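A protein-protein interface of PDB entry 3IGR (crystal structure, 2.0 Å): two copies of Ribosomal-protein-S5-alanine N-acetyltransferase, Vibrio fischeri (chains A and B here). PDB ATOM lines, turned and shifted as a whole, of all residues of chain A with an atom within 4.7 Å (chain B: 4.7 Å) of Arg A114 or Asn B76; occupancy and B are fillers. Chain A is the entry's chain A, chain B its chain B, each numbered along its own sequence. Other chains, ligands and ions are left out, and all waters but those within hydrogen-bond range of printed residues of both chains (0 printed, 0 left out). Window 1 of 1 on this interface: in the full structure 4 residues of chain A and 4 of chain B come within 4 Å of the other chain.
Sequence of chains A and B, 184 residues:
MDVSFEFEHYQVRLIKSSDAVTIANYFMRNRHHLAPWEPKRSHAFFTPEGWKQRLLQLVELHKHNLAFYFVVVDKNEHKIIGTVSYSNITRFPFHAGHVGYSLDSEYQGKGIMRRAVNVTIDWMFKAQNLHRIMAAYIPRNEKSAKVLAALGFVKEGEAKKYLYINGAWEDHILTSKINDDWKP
The guanidinium group of Arg A114 is in hydrogen-bond range of the side-chain amide oxygen of Asn B76, at 3.1 Å. The backbone carbonyl oxygen (O) of Asn B76 lies within hydrogen-bond range of the guanidinium group (NH1) of Arg A115 (2.9 Å).
O of His B9 is in hydrogen-bond range of N of Lys B75, 3.0 Å away. The side-chain carboxylate (OD1) of Asp B74 is in hydrogen-bond range of the backbone NH (N) of Asn B76 (2.8 Å).
CD of Arg A114 touches O of Glu B8, at 3.7 Å. NH2 of Arg A114 touches CB of His B9, 3.6 Å away. CG of Glu B8 touches O of Ala A150 (3.5 Å).
Arg A114 touches just these residues of chain B: Glu B8, His B9 and Asn B76. Of the printed residues of chain A, Glu B8 touches Arg A114 and Ala A150. Of the printed residues of chain A, His B9 touches Arg A114. Of the printed residues of chain B, Ala A150 touches Glu B8. The nearest residue of chain B that does not touch Arg A114 is Lys B75 (4.4 Å). The nearest printed residue of chain B that does not touch Arg A115 is Glu B77 (4.3 Å).
Of the 7 printed residues of chain B, 3 touch a printed residue of chain A. Hydrophobic or aromatic side chains of chain B that line the printed part of chain A: His B9. Along chain B the printed residues that touch a printed residue of chain A span positions 8 to 76. Printed residues of chain A that touch a printed residue of chain B: Arg A114, Arg A115 and Ala A150. Hydrophobic or aromatic side chains of chain A within 4 Å of the printed part of chain B: Ala A150. Among the printed residues, no Asp or Glu carboxylate lies within 4 Å of a Lys or Arg side-chain nitrogen of the other chain.
No position is printed for both chains. Of the 5 pairs that touch across the chains among the printed residues, none has its exchanged pair printed and touching as well.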
ATOM      1  N   GLY A 111     -25.699  -9.132 -20.797  1.00  0.00           N
ATOM      2  CA  GLY A 111     -25.478  -9.420 -19.383  1.00  0.00           C
ATOM      3  C   GLY A 111     -24.523  -8.454 -18.688  1.00  0.00           C
ATOM      4  O   GLY A 111     -24.004  -8.751 -17.605  1.00  0.00           O
ATOM      5  N   ILE A 112     -24.278  -7.299 -19.298  1.00  0.00           N
ATOM      6  CA  ILE A 112     -23.289  -6.376 -18.738  1.00  0.00           C
ATOM      7  C   ILE A 112     -23.803  -5.836 -17.399  1.00  0.00           C
ATOM      8  O   ILE A 112     -23.035  -5.693 -16.452  1.00  0.00           O
ATOM      9  CB  ILE A 112     -22.935  -5.229 -19.717  1.00  0.00           C
ATOM     10  CG1 ILE A 112     -22.213  -5.787 -20.961  1.00  0.00           C
ATOM     11  CG2 ILE A 112     -22.078  -4.158 -19.044  1.00  0.00           C
ATOM     12  CD1 ILE A 112     -22.290  -4.885 -22.149  1.00  0.00           C
ATOM     13  N   MET A 113     -25.102  -5.553 -17.324  1.00  0.00           N
ATOM     14  CA  MET A 113     -25.673  -4.960 -16.132  1.00  0.00           C
ATOM     15  C   MET A 113     -25.613  -5.947 -14.964  1.00  0.00           C
ATOM     16  O   MET A 113     -25.236  -5.584 -13.851  1.00  0.00           O
ATOM     17  CB  MET A 113     -27.109  -4.513 -16.395  1.00  0.00           C
ATOM     18  CG  MET A 113     -27.657  -3.583 -15.328  1.00  0.00           C
ATOM     19  SD  MET A 113     -27.101  -1.720 -15.591  1.00  0.00           S
ATOM     20  CE  MET A 113     -25.221  -1.755 -15.004  1.00  0.00           C
ATOM     21  N   ARG A 114     -26.020  -7.184 -15.224  1.00  0.00           N
ATOM     22  CA  ARG A 114     -25.967  -8.248 -14.232  1.00  0.00           C
ATOM     23  C   ARG A 114     -24.560  -8.409 -13.634  1.00  0.00           C
ATOM     24  O   ARG A 114     -24.407  -8.416 -12.403  1.00  0.00           O
ATOM     25  CB  ARG A 114     -26.437  -9.567 -14.847  1.00  0.00           C
ATOM     26  CG  ARG A 114     -26.525 -10.712 -13.848  1.00  0.00           C
ATOM     27  CD  ARG A 114     -26.616 -12.054 -14.555  1.00  0.00           C
ATOM     28  NE  ARG A 114     -25.401 -12.363 -15.311  1.00  0.00           N
ATOM     29  CZ  ARG A 114     -25.357 -12.554 -16.625  1.00  0.00           C
ATOM     30  NH1 ARG A 114     -26.458 -12.492 -17.348  1.00  0.00           N
ATOM     31  NH2 ARG A 114     -24.213 -12.832 -17.208  1.00  0.00           N
ATOM     32  N   ARG A 115     -23.544  -8.509 -14.492  1.00  0.00           N
ATOM     33  CA  ARG A 115     -22.154  -8.627 -14.025  1.00  0.00           C
ATOM     34  C   ARG A 115     -21.681  -7.416 -13.242  1.00  0.00           C
ATOM     35  O   ARG A 115     -21.034  -7.569 -12.201  1.00  0.00           O
ATOM     36  CB  ARG A 115     -21.165  -8.897 -15.178  1.00  0.00           C
ATOM     37  CG  ARG A 115     -21.415 -10.161 -15.991  1.00  0.00           C
ATOM     38  CD  ARG A 115     -20.231 -10.430 -16.977  1.00  0.00           C
ATOM     39  NE  ARG A 115     -19.033 -10.935 -16.283  1.00  0.00           N
ATOM     40  CZ  ARG A 115     -18.003 -11.552 -16.878  1.00  0.00           C
ATOM     41  NH1 ARG A 115     -17.984 -11.730 -18.189  1.00  0.00           N
ATOM     42  NH2 ARG A 115     -16.979 -11.991 -16.161  1.00  0.00           N
ATOM     43  N   ALA A 116     -21.987  -6.214 -13.745  1.00  0.00           N
ATOM     44  CA  ALA A 116     -21.593  -4.966 -13.072  1.00  0.00           C
ATOM     45  C   ALA A 116     -22.186  -4.851 -11.667  1.00  0.00           C
ATOM     46  O   ALA A 116     -21.487  -4.496 -10.708  1.00  0.00           O
ATOM     47  CB  ALA A 116     -21.974  -3.735 -13.938  1.00  0.00           C
ATOM     48  N   VAL A 117     -23.471  -5.172 -11.547  1.00  0.00           N
ATOM     49  CA  VAL A 117     -24.181  -5.088 -10.268  1.00  0.00           C
ATOM     50  C   VAL A 117     -23.726  -6.210  -9.334  1.00  0.00           C
ATOM     51  O   VAL A 117     -23.538  -5.976  -8.146  1.00  0.00           O
ATOM     52  CB  VAL A 117     -25.713  -5.157 -10.437  1.00  0.00           C
ATOM     53  CG1 VAL A 117     -26.416  -5.193  -9.085  1.00  0.00           C
ATOM     54  CG2 VAL A 117     -26.244  -3.961 -11.253  1.00  0.00           C
ATOM     55  N   ASN A 118     -23.557  -7.426  -9.869  1.00  0.00           N
ATOM     56  CA  ASN A 118     -23.100  -8.561  -9.060  1.00  0.00           C
ATOM     57  C   ASN A 118     -21.757  -8.321  -8.392  1.00  0.00           C
ATOM     58  O   ASN A 118     -21.564  -8.660  -7.216  1.00  0.00           O
ATOM     59  CB  ASN A 118     -22.987  -9.831  -9.897  1.00  0.00           C
ATOM     60  CG  ASN A 118     -22.893 -11.076  -9.045  1.00  0.00           C
ATOM     61  OD1 ASN A 118     -23.085 -11.029  -7.834  1.00  0.00           O
ATOM     62  ND2 ASN A 118     -22.617 -12.204  -9.680  1.00  0.00           N
ATOM     63  N   VAL A 147     -32.458  -8.912 -14.093  1.00  0.00           N
ATOM     64  CA  VAL A 147     -31.188  -8.651 -13.451  1.00  0.00           C
ATOM     65  C   VAL A 147     -31.288  -9.009 -11.965  1.00  0.00           C
ATOM     66  O   VAL A 147     -30.524  -9.839 -11.474  1.00  0.00           O
ATOM     67  CB  VAL A 147     -30.750  -7.173 -13.619  1.00  0.00           C
ATOM     68  CG1 VAL A 147     -29.659  -6.816 -12.607  1.00  0.00           C
ATOM     69  CG2 VAL A 147     -30.274  -6.920 -15.047  1.00  0.00           C
ATOM     70  N   ALA A 150     -31.722 -12.632 -11.183  1.00  0.00           N
ATOM     71  CA  ALA A 150     -30.516 -13.409 -11.467  1.00  0.00           C
ATOM     72  C   ALA A 150     -29.475 -13.268 -10.347  1.00  0.00           C
ATOM     73  O   ALA A 150     -28.624 -14.155 -10.156  1.00  0.00           O
ATOM     74  CB  ALA A 150     -29.915 -13.012 -12.811  1.00  0.00           C
ATOM     75  N   LEU A 151     -29.561 -12.161  -9.612  1.00  0.00           N
ATOM     76  CA  LEU A 151     -28.608 -11.840  -8.558  1.00  0.00           C
ATOM     77  C   LEU A 151     -29.102 -12.234  -7.179  1.00  0.00           C
ATOM     78  O   LEU A 151     -28.454 -11.940  -6.168  1.00  0.00           O
ATOM     79  CB  LEU A 151     -28.283 -10.346  -8.616  1.00  0.00           C
ATOM     80  CG  LEU A 151     -27.519  -9.990  -9.896  1.00  0.00           C
ATOM     81  CD1 LEU A 151     -27.183  -8.515  -9.893  1.00  0.00           C
ATOM     82  CD2 LEU A 151     -26.258 -10.819  -9.985  1.00  0.00           C
ATOM     83  N   GLU B   8     -29.144 -17.220 -13.367  1.00  0.00           N
ATOM     84  CA  GLU B   8     -27.961 -16.477 -12.927  1.00  0.00           C
ATOM     85  C   GLU B   8     -27.109 -16.150 -14.159  1.00  0.00           C
ATOM     86  O   GLU B   8     -27.616 -15.533 -15.101  1.00  0.00           O
ATOM     87  CB  GLU B   8     -27.186 -17.254 -11.853  1.00  0.00           C
ATOM     88  CG  GLU B   8     -28.022 -17.613 -10.630  1.00  0.00           C
ATOM     89  CD  GLU B   8     -27.230 -18.340  -9.553  1.00  0.00           C
ATOM     90  OE1 GLU B   8     -26.055 -18.689  -9.767  1.00  0.00           O
ATOM     91  OE2 GLU B   8     -27.787 -18.566  -8.470  1.00  0.00           O
ATOM     92  N   HIS B   9     -25.845 -16.569 -14.173  1.00  0.00           N
ATOM     93  CA  HIS B   9     -25.008 -16.394 -15.354  1.00  0.00           C
ATOM     94  C   HIS B   9     -24.649 -17.707 -16.035  1.00  0.00           C
ATOM     95  O   HIS B   9     -23.575 -17.837 -16.632  1.00  0.00           O
ATOM     96  CB  HIS B   9     -23.742 -15.593 -15.021  1.00  0.00           C
ATOM     97  CG  HIS B   9     -22.889 -16.205 -13.954  1.00  0.00           C
ATOM     98  ND1 HIS B   9     -23.115 -15.994 -12.607  1.00  0.00           N
ATOM     99  CD2 HIS B   9     -21.788 -16.993 -14.031  1.00  0.00           C
ATOM    100  CE1 HIS B   9     -22.196 -16.632 -11.903  1.00  0.00           C
ATOM    101  NE2 HIS B   9     -21.376 -17.242 -12.743  1.00  0.00           N
ATOM    102  N   ASP B  74     -20.797 -21.484 -18.331  1.00  0.00           N
ATOM    103  CA  ASP B  74     -20.615 -20.232 -17.605  1.00  0.00           C
ATOM    104  C   ASP B  74     -20.501 -19.133 -18.646  1.00  0.00           C
ATOM    105  O   ASP B  74     -19.457 -18.971 -19.275  1.00  0.00           O
ATOM    106  CB  ASP B  74     -19.371 -20.290 -16.716  1.00  0.00           C
ATOM    107  CG  ASP B  74     -19.167 -19.024 -15.900  1.00  0.00           C
ATOM    108  OD1 ASP B  74     -19.734 -17.956 -16.256  1.00  0.00           O
ATOM    109  OD2 ASP B  74     -18.434 -19.100 -14.889  1.00  0.00           O
ATOM    110  N   LYS B  75     -21.593 -18.412 -18.852  1.00  0.00           N
ATOM    111  CA  LYS B  75     -21.651 -17.326 -19.829  1.00  0.00           C
ATOM    112  C   LYS B  75     -20.699 -16.178 -19.518  1.00  0.00           C
ATOM    113  O   LYS B  75     -20.348 -15.413 -20.426  1.00  0.00           O
ATOM    114  CB  LYS B  75     -23.072 -16.777 -19.927  1.00  0.00           C
ATOM    115  CG  LYS B  75     -24.028 -17.709 -20.663  1.00  0.00           C
ATOM    116  CD  LYS B  75     -25.435 -17.659 -20.061  1.00  0.00           C
ATOM    117  CE  LYS B  75     -26.066 -16.291 -20.141  1.00  0.00           C
ATOM    118  NZ  LYS B  75     -27.401 -16.263 -19.467  1.00  0.00           N
ATOM    119  N   ASN B  76     -20.311 -16.027 -18.249  1.00  0.00           N
ATOM    120  CA  ASN B  76     -19.294 -15.017 -17.885  1.00  0.00           C
ATOM    121  C   ASN B  76     -17.897 -15.377 -18.396  1.00  0.00           C
ATOM    122  O   ASN B  76     -17.107 -14.480 -18.731  1.00  0.00           O
ATOM    123  CB  ASN B  76     -19.215 -14.824 -16.368  1.00  0.00           C
ATOM    124  CG  ASN B  76     -20.409 -14.083 -15.802  1.00  0.00           C
ATOM    125  OD1 ASN B  76     -21.253 -13.565 -16.541  1.00  0.00           O
ATOM    126  ND2 ASN B  76     -20.483 -14.025 -14.471  1.00  0.00           N
ATOM    127  N   GLU B  77     -17.596 -16.679 -18.405  1.00  0.00           N
ATOM    128  CA  GLU B  77     -16.253 -17.189 -18.701  1.00  0.00           C
ATOM    129  C   GLU B  77     -16.182 -17.867 -20.066  1.00  0.00           C
ATOM    130  O   GLU B  77     -15.088 -18.206 -20.543  1.00  0.00           O
ATOM    131  CB  GLU B  77     -15.808 -18.198 -17.626  1.00  0.00           C
ATOM    132  CG  GLU B  77     -15.548 -17.598 -16.242  1.00  0.00           C
ATOM    133  CD  GLU B  77     -14.482 -16.521 -16.246  1.00  0.00           C
ATOM    134  OE1 GLU B  77     -13.494 -16.647 -17.009  1.00  0.00           O
ATOM    135  OE2 GLU B  77     -14.628 -15.542 -15.479  1.00  0.00           O
ATOM    136  N   HIS B  78     -17.354 -18.077 -20.672  1.00  0.00           N
ATOM    137  CA  HIS B  78     -17.491 -18.749 -21.977  1.00  0.00           C
ATOM    138  C   HIS B  78     -16.829 -20.107 -21.956  1.00  0.00           C
ATOM    139  O   HIS B  78     -16.034 -20.438 -22.834  1.00  0.00           O
ATOM    140  CB  HIS B  78     -16.929 -17.886 -23.112  1.00  0.00           C
ATOM    141  CG  HIS B  78     -17.454 -16.492 -23.096  1.00  0.00           C
ATOM    142  ND1 HIS B  78     -16.683 -15.414 -22.723  1.00  0.00           N
ATOM    143  CD2 HIS B  78     -18.692 -16.004 -23.344  1.00  0.00           C
ATOM    144  CE1 HIS B  78     -17.418 -14.318 -22.765  1.00  0.00           C
ATOM    145  NE2 HIS B  78     -18.641 -14.648 -23.138  1.00  0.00           N
